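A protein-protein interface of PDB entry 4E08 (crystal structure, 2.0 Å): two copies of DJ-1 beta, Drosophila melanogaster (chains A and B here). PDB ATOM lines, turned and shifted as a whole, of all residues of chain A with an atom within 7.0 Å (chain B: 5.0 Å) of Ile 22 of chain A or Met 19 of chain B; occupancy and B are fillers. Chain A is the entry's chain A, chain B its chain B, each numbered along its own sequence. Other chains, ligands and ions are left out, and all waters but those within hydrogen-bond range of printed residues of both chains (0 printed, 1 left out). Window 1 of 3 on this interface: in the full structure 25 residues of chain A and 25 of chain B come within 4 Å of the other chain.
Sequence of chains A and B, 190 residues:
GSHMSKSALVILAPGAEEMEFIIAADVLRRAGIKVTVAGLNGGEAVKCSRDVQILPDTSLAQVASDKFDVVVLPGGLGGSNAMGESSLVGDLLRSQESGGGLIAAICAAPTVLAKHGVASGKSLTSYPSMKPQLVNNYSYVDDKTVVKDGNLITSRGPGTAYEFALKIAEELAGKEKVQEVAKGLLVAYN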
ATOM      1  N   VAL A  10     -11.642 -26.398  -6.144  1.00  0.00           N
ATOM      2  CA  VAL A  10     -10.658 -25.953  -7.117  1.00  0.00           C
ATOM      3  C   VAL A  10      -9.302 -25.853  -6.445  1.00  0.00           C
ATOM      4  O   VAL A  10      -9.102 -25.009  -5.509  1.00  0.00           O
ATOM      5  CB  VAL A  10     -11.058 -24.615  -7.785  1.00  0.00           C
ATOM      6  CG1 VAL A  10     -10.071 -24.249  -8.892  1.00  0.00           C
ATOM      7  CG2 VAL A  10     -12.475 -24.706  -8.330  1.00  0.00           C
ATOM      8  N   GLU A  17      -1.599 -21.799 -13.839  1.00  0.00           N
ATOM      9  CA  GLU A  17      -2.078 -20.825 -14.819  1.00  0.00           C
ATOM     10  C   GLU A  17      -3.307 -20.081 -14.252  1.00  0.00           C
ATOM     11  O   GLU A  17      -4.443 -20.598 -14.250  1.00  0.00           O
ATOM     12  CB  GLU A  17      -2.390 -21.514 -16.170  1.00  0.00           C
ATOM     13  CG  GLU A  17      -1.680 -20.744 -17.337  1.00  0.00           C
ATOM     14  CD  GLU A  17      -2.118 -19.286 -17.380  1.00  0.00           C
ATOM     15  OE1 GLU A  17      -3.327 -19.061 -17.106  1.00  0.00           O
ATOM     16  OE2 GLU A  17      -1.262 -18.378 -17.645  1.00  0.00           O
ATOM     17  N   GLU A  18      -3.037 -18.883 -13.755  1.00  0.00           N
ATOM     18  CA  GLU A  18      -4.021 -18.033 -13.105  1.00  0.00           C
ATOM     19  C   GLU A  18      -5.292 -17.748 -13.935  1.00  0.00           C
ATOM     20  O   GLU A  18      -6.362 -17.589 -13.363  1.00  0.00           O
ATOM     21  CB  GLU A  18      -3.376 -16.695 -12.675  1.00  0.00           C
ATOM     22  CG  GLU A  18      -2.530 -15.977 -13.708  1.00  0.00           C
ATOM     23  CD  GLU A  18      -1.042 -16.352 -13.613  1.00  0.00           C
ATOM     24  OE1 GLU A  18      -0.244 -15.559 -13.060  1.00  0.00           O
ATOM     25  OE2 GLU A  18      -0.698 -17.466 -14.069  1.00  0.00           O
ATOM     26  N   MET A  19      -5.154 -17.620 -15.255  1.00  0.00           N
ATOM     27  CA  MET A  19      -6.311 -17.382 -16.124  1.00  0.00           C
ATOM     28  C   MET A  19      -7.208 -18.571 -16.063  1.00  0.00           C
ATOM     29  O   MET A  19      -8.392 -18.430 -15.797  1.00  0.00           O
ATOM     30  CB  MET A  19      -5.921 -17.081 -17.578  1.00  0.00           C
ATOM     31  CG  MET A  19      -5.062 -15.822 -17.698  1.00  0.00           C
ATOM     32  SD  MET A  19      -4.672 -15.479 -19.413  1.00  0.00           S
ATOM     33  CE  MET A  19      -3.733 -16.989 -19.757  1.00  0.00           C
ATOM     34  N   GLU A  20      -6.647 -19.749 -16.311  1.00  0.00           N
ATOM     35  CA  GLU A  20      -7.425 -20.990 -16.279  1.00  0.00           C
ATOM     36  C   GLU A  20      -8.132 -21.179 -14.923  1.00  0.00           C
ATOM     37  O   GLU A  20      -9.310 -21.492 -14.853  1.00  0.00           O
ATOM     38  CB  GLU A  20      -6.481 -22.168 -16.532  1.00  0.00           C
ATOM     39  CG  GLU A  20      -6.169 -22.315 -18.001  1.00  0.00           C
ATOM     40  CD  GLU A  20      -5.010 -23.247 -18.253  1.00  0.00           C
ATOM     41  OE1 GLU A  20      -4.673 -24.070 -17.369  1.00  0.00           O
ATOM     42  OE2 GLU A  20      -4.432 -23.137 -19.352  1.00  0.00           O
ATOM     43  N   PHE A  21      -7.353 -21.030 -13.862  1.00  0.00           N
ATOM     44  CA  PHE A  21      -7.852 -21.053 -12.481  1.00  0.00           C
ATOM     45  C   PHE A  21      -9.026 -20.086 -12.245  1.00  0.00           C
ATOM     46  O   PHE A  21     -10.061 -20.490 -11.695  1.00  0.00           O
ATOM     47  CB  PHE A  21      -6.751 -20.703 -11.445  1.00  0.00           C
ATOM     48  CG  PHE A  21      -7.340 -20.339 -10.102  1.00  0.00           C
ATOM     49  CD1 PHE A  21      -7.909 -21.330  -9.293  1.00  0.00           C
ATOM     50  CD2 PHE A  21      -7.433 -19.002  -9.693  1.00  0.00           C
ATOM     51  CE1 PHE A  21      -8.517 -20.998  -8.062  1.00  0.00           C
ATOM     52  CE2 PHE A  21      -8.028 -18.654  -8.451  1.00  0.00           C
ATOM     53  CZ  PHE A  21      -8.576 -19.674  -7.650  1.00  0.00           C
ATOM     54  N   ILE A  22      -8.823 -18.814 -12.610  1.00  0.00           N
ATOM     55  CA  ILE A  22      -9.768 -17.742 -12.262  1.00  0.00           C
ATOM     56  C   ILE A  22     -11.076 -17.952 -13.045  1.00  0.00           C
ATOM     57  O   ILE A  22     -12.169 -17.798 -12.503  1.00  0.00           O
ATOM     58  CB  ILE A  22      -9.147 -16.316 -12.459  1.00  0.00           C
ATOM     59  CG1 ILE A  22      -9.902 -15.270 -11.677  1.00  0.00           C
ATOM     60  CG2 ILE A  22      -9.171 -15.840 -13.933  1.00  0.00           C
ATOM     61  CD1 ILE A  22      -9.893 -15.581 -10.155  1.00  0.00           C
ATOM     62  N   ILE A  23     -10.942 -18.370 -14.302  1.00  0.00           N
ATOM     63  CA  ILE A  23     -12.112 -18.674 -15.116  1.00  0.00           C
ATOM     64  C   ILE A  23     -12.985 -19.803 -14.553  1.00  0.00           C
ATOM     65  O   ILE A  23     -14.164 -19.627 -14.469  1.00  0.00           O
ATOM     66  CB  ILE A  23     -11.738 -18.927 -16.583  1.00  0.00           C
ATOM     67  CG1 ILE A  23     -11.196 -17.613 -17.205  1.00  0.00           C
ATOM     68  CG2 ILE A  23     -12.960 -19.485 -17.364  1.00  0.00           C
ATOM     69  CD1 ILE A  23     -10.488 -17.804 -18.544  1.00  0.00           C
ATOM     70  N   ALA A  24     -12.385 -20.942 -14.202  1.00  0.00           N
ATOM     71  CA  ALA A  24     -13.072 -22.039 -13.534  1.00  0.00           C
ATOM     72  C   ALA A  24     -13.673 -21.591 -12.192  1.00  0.00           C
ATOM     73  O   ALA A  24     -14.841 -21.839 -11.953  1.00  0.00           O
ATOM     74  CB  ALA A  24     -12.122 -23.255 -13.348  1.00  0.00           C
ATOM     75  N   ALA A  25     -12.929 -20.900 -11.332  1.00  0.00           N
ATOM     76  CA  ALA A  25     -13.551 -20.446 -10.073  1.00  0.00           C
ATOM     77  C   ALA A  25     -14.726 -19.512 -10.303  1.00  0.00           C
ATOM     78  O   ALA A  25     -15.753 -19.668  -9.672  1.00  0.00           O
ATOM     79  CB  ALA A  25     -12.574 -19.785  -9.159  1.00  0.00           C
ATOM     80  N   ASP A  26     -14.555 -18.541 -11.210  1.00  0.00           N
ATOM     81  CA  ASP A  26     -15.478 -17.416 -11.306  1.00  0.00           C
ATOM     82  C   ASP A  26     -16.718 -17.904 -12.049  1.00  0.00           C
ATOM     83  O   ASP A  26     -17.805 -17.597 -11.624  1.00  0.00           O
ATOM     84  CB  ASP A  26     -14.766 -16.268 -12.029  1.00  0.00           C
ATOM     85  CG  ASP A  26     -15.617 -15.019 -12.185  1.00  0.00           C
ATOM     86  OD1 ASP A  26     -16.767 -15.087 -12.600  1.00  0.00           O
ATOM     87  OD2 ASP A  26     -15.116 -13.912 -11.899  1.00  0.00           O
ATOM     88  N   VAL A  27     -16.536 -18.698 -13.119  1.00  0.00           N
ATOM     89  CA  VAL A  27     -17.672 -19.213 -13.901  1.00  0.00           C
ATOM     90  C   VAL A  27     -18.528 -20.159 -13.046  1.00  0.00           C
ATOM     91  O   VAL A  27     -19.753 -20.100 -13.107  1.00  0.00           O
ATOM     92  CB  VAL A  27     -17.234 -19.914 -15.227  1.00  0.00           C
ATOM     93  CG1 VAL A  27     -18.388 -20.587 -15.903  1.00  0.00           C
ATOM     94  CG2 VAL A  27     -16.584 -18.887 -16.140  1.00  0.00           C
ATOM     95  N   LEU A  28     -17.874 -20.965 -12.221  1.00  0.00           N
ATOM     96  CA  LEU A  28     -18.585 -21.915 -11.380  1.00  0.00           C
ATOM     97  C   LEU A  28     -19.449 -21.204 -10.332  1.00  0.00           C
ATOM     98  O   LEU A  28     -20.588 -21.608 -10.069  1.00  0.00           O
ATOM     99  CB  LEU A  28     -17.596 -22.906 -10.742  1.00  0.00           C
ATOM    100  CG  LEU A  28     -17.032 -23.982 -11.717  1.00  0.00           C
ATOM    101  CD1 LEU A  28     -16.059 -24.930 -11.033  1.00  0.00           C
ATOM    102  CD2 LEU A  28     -18.171 -24.802 -12.379  1.00  0.00           C
ATOM    103  N   ARG A  30     -20.617 -18.098 -10.721  1.00  0.00           N
ATOM    104  CA  ARG A  30     -21.709 -17.473 -11.520  1.00  0.00           C
ATOM    105  C   ARG A  30     -22.866 -18.439 -11.694  1.00  0.00           C
ATOM    106  O   ARG A  30     -24.018 -18.029 -11.684  1.00  0.00           O
ATOM    107  CB  ARG A  30     -21.216 -17.001 -12.910  1.00  0.00           C
ATOM    108  CG  ARG A  30     -20.544 -15.637 -12.906  1.00  0.00           C
ATOM    109  CD  ARG A  30     -19.779 -15.297 -14.214  1.00  0.00           C
ATOM    110  NE  ARG A  30     -19.021 -14.063 -14.032  1.00  0.00           N
ATOM    111  CZ  ARG A  30     -19.358 -12.882 -14.547  1.00  0.00           C
ATOM    112  NH1 ARG A  30     -20.430 -12.776 -15.326  1.00  0.00           N
ATOM    113  NH2 ARG A  30     -18.594 -11.803 -14.294  1.00  0.00           N
ATOM    114  N   ILE A  54      -2.518 -15.087  -5.439  1.00  0.00           N
ATOM    115  CA  ILE A  54      -3.949 -15.257  -5.181  1.00  0.00           C
ATOM    116  C   ILE A  54      -4.103 -15.887  -3.824  1.00  0.00           C
ATOM    117  O   ILE A  54      -3.440 -16.871  -3.521  1.00  0.00           O
ATOM    118  CB  ILE A  54      -4.614 -16.134  -6.278  1.00  0.00           C
ATOM    119  CG1 ILE A  54      -4.439 -15.474  -7.654  1.00  0.00           C
ATOM    120  CG2 ILE A  54      -6.133 -16.371  -5.994  1.00  0.00           C
ATOM    121  CD1 ILE A  54      -5.085 -16.252  -8.790  1.00  0.00           C
ATOM    122  N   PRO A  74      -6.660 -26.803 -12.310  1.00  0.00           N
ATOM    123  CA  PRO A  74      -6.201 -25.839 -13.306  1.00  0.00           C
ATOM    124  C   PRO A  74      -4.880 -26.351 -13.909  1.00  0.00           C
ATOM    125  O   PRO A  74      -4.204 -27.165 -13.269  1.00  0.00           O
ATOM    126  CB  PRO A  74      -5.959 -24.552 -12.467  1.00  0.00           C
ATOM    127  CG  PRO A  74      -6.944 -24.663 -11.354  1.00  0.00           C
ATOM    128  CD  PRO A  74      -6.852 -26.168 -10.994  1.00  0.00           C
ATOM    129  N   TYR A 162     -12.969 -20.963 -20.963  1.00  0.00           N
ATOM    130  CA  TYR A 162     -14.364 -20.602 -20.759  1.00  0.00           C
ATOM    131  C   TYR A 162     -15.239 -21.793 -21.095  1.00  0.00           C
ATOM    132  O   TYR A 162     -16.127 -22.113 -20.343  1.00  0.00           O
ATOM    133  CB  TYR A 162     -14.802 -19.361 -21.549  1.00  0.00           C
ATOM    134  CG  TYR A 162     -14.469 -18.063 -20.848  1.00  0.00           C
ATOM    135  CD1 TYR A 162     -15.114 -17.686 -19.687  1.00  0.00           C
ATOM    136  CD2 TYR A 162     -13.504 -17.206 -21.385  1.00  0.00           C
ATOM    137  CE1 TYR A 162     -14.787 -16.479 -19.045  1.00  0.00           C
ATOM    138  CE2 TYR A 162     -13.179 -16.012 -20.771  1.00  0.00           C
ATOM    139  CZ  TYR A 162     -13.792 -15.663 -19.599  1.00  0.00           C
ATOM    140  OH  TYR A 162     -13.391 -14.470 -19.044  1.00  0.00           O
ATOM    141  N   LEU A 185     -21.739 -13.642 -19.760  1.00  0.00           N
ATOM    142  CA  LEU A 185     -20.291 -13.631 -20.098  1.00  0.00           C
ATOM    143  C   LEU A 185     -19.927 -13.060 -21.470  1.00  0.00           C
ATOM    144  O   LEU A 185     -18.750 -12.727 -21.725  1.00  0.00           O
ATOM    145  CB  LEU A 185     -19.760 -15.069 -20.035  1.00  0.00           C
ATOM    146  CG  LEU A 185     -19.698 -15.764 -18.660  1.00  0.00           C
ATOM    147  CD1 LEU A 185     -19.323 -17.222 -18.789  1.00  0.00           C
ATOM    148  CD2 LEU A 185     -18.755 -15.045 -17.712  1.00  0.00           C
ATOM    149  N   GLU B  17     -13.778  -7.279 -11.872  1.00  0.00           N
ATOM    150  CA  GLU B  17     -14.117  -8.522 -12.522  1.00  0.00           C
ATOM    151  C   GLU B  17     -12.781  -9.260 -12.669  1.00  0.00           C
ATOM    152  O   GLU B  17     -11.902  -8.855 -13.478  1.00  0.00           O
ATOM    153  CB  GLU B  17     -14.750  -8.221 -13.892  1.00  0.00           C
ATOM    154  CG  GLU B  17     -15.548  -9.364 -14.444  1.00  0.00           C
ATOM    155  CD  GLU B  17     -14.641 -10.519 -14.824  1.00  0.00           C
ATOM    156  OE1 GLU B  17     -14.010 -10.441 -15.908  1.00  0.00           O
ATOM    157  OE2 GLU B  17     -14.526 -11.468 -14.035  1.00  0.00           O
ATOM    158  N   GLU B  18     -12.608 -10.335 -11.898  1.00  0.00           N
ATOM    159  CA  GLU B  18     -11.258 -10.923 -11.769  1.00  0.00           C
ATOM    160  C   GLU B  18     -10.735 -11.590 -13.035  1.00  0.00           C
ATOM    161  O   GLU B  18      -9.522 -11.689 -13.236  1.00  0.00           O
ATOM    162  CB  GLU B  18     -11.161 -11.880 -10.569  1.00  0.00           C
ATOM    163  CG  GLU B  18     -12.334 -12.863 -10.417  1.00  0.00           C
ATOM    164  CD  GLU B  18     -13.471 -12.238  -9.613  1.00  0.00           C
ATOM    165  OE1 GLU B  18     -13.619 -12.553  -8.429  1.00  0.00           O
ATOM    166  OE2 GLU B  18     -14.180 -11.377 -10.181  1.00  0.00           O
ATOM    167  N   MET B  19     -11.646 -12.096 -13.862  1.00  0.00           N
ATOM    168  CA  MET B  19     -11.251 -12.804 -15.066  1.00  0.00           C
ATOM    169  C   MET B  19     -10.578 -11.826 -16.022  1.00  0.00           C
ATOM    170  O   MET B  19      -9.463 -12.090 -16.472  1.00  0.00           O
ATOM    171  CB  MET B  19     -12.467 -13.443 -15.716  1.00  0.00           C
ATOM    172  CG  MET B  19     -12.997 -14.622 -14.870  1.00  0.00           C
ATOM    173  SD  MET B  19     -14.394 -15.512 -15.626  1.00  0.00           S
ATOM    174  CE  MET B  19     -15.564 -14.136 -15.712  1.00  0.00           C
ATOM    175  N   GLU B  20     -11.228 -10.680 -16.263  1.00  0.00           N
ATOM    176  CA  GLU B  20     -10.749  -9.673 -17.225  1.00  0.00           C
ATOM    177  C   GLU B  20      -9.445  -9.117 -16.687  1.00  0.00           C
ATOM    178  O   GLU B  20      -8.478  -8.890 -17.424  1.00  0.00           O
ATOM    179  CB  GLU B  20     -11.766  -8.520 -17.360  1.00  0.00           C
ATOM    180  CG  GLU B  20     -13.054  -8.837 -18.141  1.00  0.00           C
ATOM    181  CD  GLU B  20     -14.180  -7.893 -17.760  1.00  0.00           C
ATOM    182  OE1 GLU B  20     -13.883  -6.823 -17.179  1.00  0.00           O
ATOM    183  OE2 GLU B  20     -15.344  -8.214 -18.028  1.00  0.00           O
ATOM    184  N   PHE B  21      -9.416  -8.911 -15.375  1.00  0.00           N
ATOM    185  CA  PHE B  21      -8.187  -8.497 -14.754  1.00  0.00           C
ATOM    186  C   PHE B  21      -7.029  -9.489 -14.984  1.00  0.00           C
ATOM    187  O   PHE B  21      -5.914  -9.078 -15.427  1.00  0.00           O
ATOM    188  CB  PHE B  21      -8.331  -8.276 -13.245  1.00  0.00           C
ATOM    189  CG  PHE B  21      -7.013  -8.196 -12.585  1.00  0.00           C
ATOM    190  CD1 PHE B  21      -6.235  -7.071 -12.740  1.00  0.00           C
ATOM    191  CD2 PHE B  21      -6.482  -9.292 -11.911  1.00  0.00           C
ATOM    192  CE1 PHE B  21      -4.963  -7.003 -12.193  1.00  0.00           C
ATOM    193  CE2 PHE B  21      -5.194  -9.232 -11.365  1.00  0.00           C
ATOM    194  CZ  PHE B  21      -4.437  -8.074 -11.521  1.00  0.00           C
ATOM    195  N   ILE B  22      -7.246 -10.767 -14.629  1.00  0.00           N
ATOM    196  CA  ILE B  22      -6.150 -11.732 -14.711  1.00  0.00           C
ATOM    197  C   ILE B  22      -5.716 -11.902 -16.187  1.00  0.00           C
ATOM    198  O   ILE B  22      -4.534 -11.944 -16.499  1.00  0.00           O
ATOM    199  CB  ILE B  22      -6.475 -13.074 -14.016  1.00  0.00           C
ATOM    200  CG1 ILE B  22      -6.188 -12.924 -12.513  1.00  0.00           C
ATOM    201  CG2 ILE B  22      -5.498 -14.161 -14.407  1.00  0.00           C
ATOM    202  CD1 ILE B  22      -6.691 -14.116 -11.583  1.00  0.00           C
ATOM    203  N   ILE B  23      -6.691 -11.992 -17.087  1.00  0.00           N
ATOM    204  CA  ILE B  23      -6.385 -12.141 -18.518  1.00  0.00           C
ATOM    205  C   ILE B  23      -5.498 -11.000 -19.023  1.00  0.00           C
ATOM    206  O   ILE B  23      -4.531 -11.261 -19.745  1.00  0.00           O
ATOM    207  CB  ILE B  23      -7.670 -12.275 -19.390  1.00  0.00           C
ATOM    208  CG1 ILE B  23      -8.393 -13.583 -19.007  1.00  0.00           C
ATOM    209  CG2 ILE B  23      -7.290 -12.250 -20.911  1.00  0.00           C
ATOM    210  CD1 ILE B  23      -9.749 -13.786 -19.647  1.00  0.00           C
ATOM    211  N   ALA B  24      -5.831  -9.754 -18.632  1.00  0.00           N
ATOM    212  CA  ALA B  24      -5.013  -8.578 -18.972  1.00  0.00           C
ATOM    213  C   ALA B  24      -3.592  -8.697 -18.442  1.00  0.00           C
ATOM    214  O   ALA B  24      -2.619  -8.504 -19.210  1.00  0.00           O
ATOM    215  CB  ALA B  24      -5.678  -7.234 -18.493  1.00  0.00           C
ATOM    216  N   VAL B  52     -12.716 -13.654  -5.205  1.00  0.00           N
ATOM    217  CA  VAL B  52     -11.336 -14.073  -5.330  1.00  0.00           C
ATOM    218  C   VAL B  52     -10.468 -12.894  -4.834  1.00  0.00           C
ATOM    219  O   VAL B  52     -10.732 -11.730  -5.149  1.00  0.00           O
ATOM    220  CB  VAL B  52     -11.017 -14.458  -6.781  1.00  0.00           C
ATOM    221  CG1 VAL B  52      -9.570 -14.907  -6.899  1.00  0.00           C
ATOM    222  CG2 VAL B  52     -11.992 -15.599  -7.250  1.00  0.00           C
ATOM    223  N   PRO B 158     -16.176 -10.599 -20.348  1.00  0.00           N
ATOM    224  CA  PRO B 158     -15.329 -11.788 -20.223  1.00  0.00           C
ATOM    225  C   PRO B 158     -15.057 -12.462 -21.584  1.00  0.00           C
ATOM    226  O   PRO B 158     -13.905 -12.838 -21.858  1.00  0.00           O
ATOM    227  CB  PRO B 158     -16.169 -12.709 -19.325  1.00  0.00           C
ATOM    228  CG  PRO B 158     -16.927 -11.743 -18.464  1.00  0.00           C
ATOM    229  CD  PRO B 158     -17.290 -10.613 -19.377  1.00  0.00           C
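Of the printed residues of chain B, Ile 22 of chain A touches Glu 18 (3.6 Å), Met 19 (3.9 Å), Ile 22 (3.4 Å) and Val 52 (3.3 Å). Met 19 of chain B touches just these residues of chain A: Ile 22 (3.9 Å), Ile 23 (3.9 Å), Asp 26 (3.5 Å), Arg 30 (3.8 Å), Tyr 162 (3.6 Å) and Leu 185 (3.9 Å). Of the printed residues of chain B, Ile 54 of chain A touches Ile 22 (3.9 Å) and Val 52 (3.8 Å). Printed residues of chain B within 4 Å of Met 19 of chain A: Ile 22 and Ile 23. Of the printed residues of chain A, Pro 158 of chain B touches Tyr 162 and Leu 185. Of the printed residues of chain B, Leu 185 of chain A touches Met 19 (3.9 Å) and Pro 158 (3.5 Å). Val 27 of chain A touches none of the printed residues of chain B.
Glu 18 of chain A touches Ile 22 of chain B. N of Met 19 of chain A touches CG2 of Ile 22 of chain B (3.6 Å). Met 19 of chain A touches Ile 23 of chain B (SD to CA, 3.9 Å). Ile 22 of chain B touches Ile 22 of chain A (CD1 to CB, 3.4 Å). Ile 22 of chain A touches Val 52 of chain B (CD1 to CG1, 3.3 Å). Met 19 of chain B touches Asp 26 of chain A. NH2 of Arg 30 of chain A touches CG of Glu 17 of chain B, 3.9 Å away. Ile 54 of chain A touches Ile 22 of chain B. Tyr 162 of chain A touches Ile 23 of chain B (OH to CD1, 3.8 Å). CD of Pro 158 of chain B touches O of Leu 185 of chain A, 3.5 Å away.
Glu 18 of chain A touches Ile 22 of chain B, and with the chains exchanged Ile 22 of chain A touches Glu 18 of chain B. Met 19 of chain A touches Ile 22 of chain B, and with the chains exchanged Ile 22 of chain A touches Met 19 of chain B. Met 19 of chain A touches Ile 23 of chain B, and with the chains exchanged Ile 23 of chain A touches Met 19 of chain B. Ile 22 of chain A touches its own counterpart, Ile 22 of chain B. Of the 20 pairs that touch across the chains among the printed residues, 7 have their exchanged pair printed and touching as well.
Of the 18 printed residues of chain A, 9 touch a printed residue of chain B. Printed residues of chain B that touch a printed residue of chain A: Glu 17, Glu 18, Met 19, Ile 22, Ile 23, Val 52 and Pro 158. Among the printed residues, no Asp or Glu carboxylate lies within 4 Å of a Lys or Arg side-chain nitrogen of the other chain.
The side-chain carboxylate (OD2) of Asp 26 of chain A lies close to the side-chain carboxylate (OE2) of Glu 17 of chain B (3.3 Å). OH of Tyr 162 of chain A lies within hydrogen-bond range of O of Pro 158 of chain B (3.3 Å). OD2 of Asp 26 of chain A lies close to OE2 of Glu 18 of chain B (3.2 Å). OH of Tyr 162 of chain A sits close to SD of Met 19 of chain B (3.7 Å).
The guanidinium group of Arg 30 of chain A is in salt-bridge range of the side-chain carboxylate of Asp 26 of chain A (2.9 Å). The side-chain carboxylate (OE1) of Glu 17 of chain A lies within hydrogen-bond range of the backbone NH (N) of Met 19 of chain A (3.0 Å). OE2 of Glu 17 of chain B sits at hydrogen-bond distance from N of Met 19 of chain B, at 3.0 Å. The side-chain carboxylate (OE1) of Glu 17 of chain B is in hydrogen-bond range of the backbone NH (N) of Glu 20 of chain B (2.8 Å).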
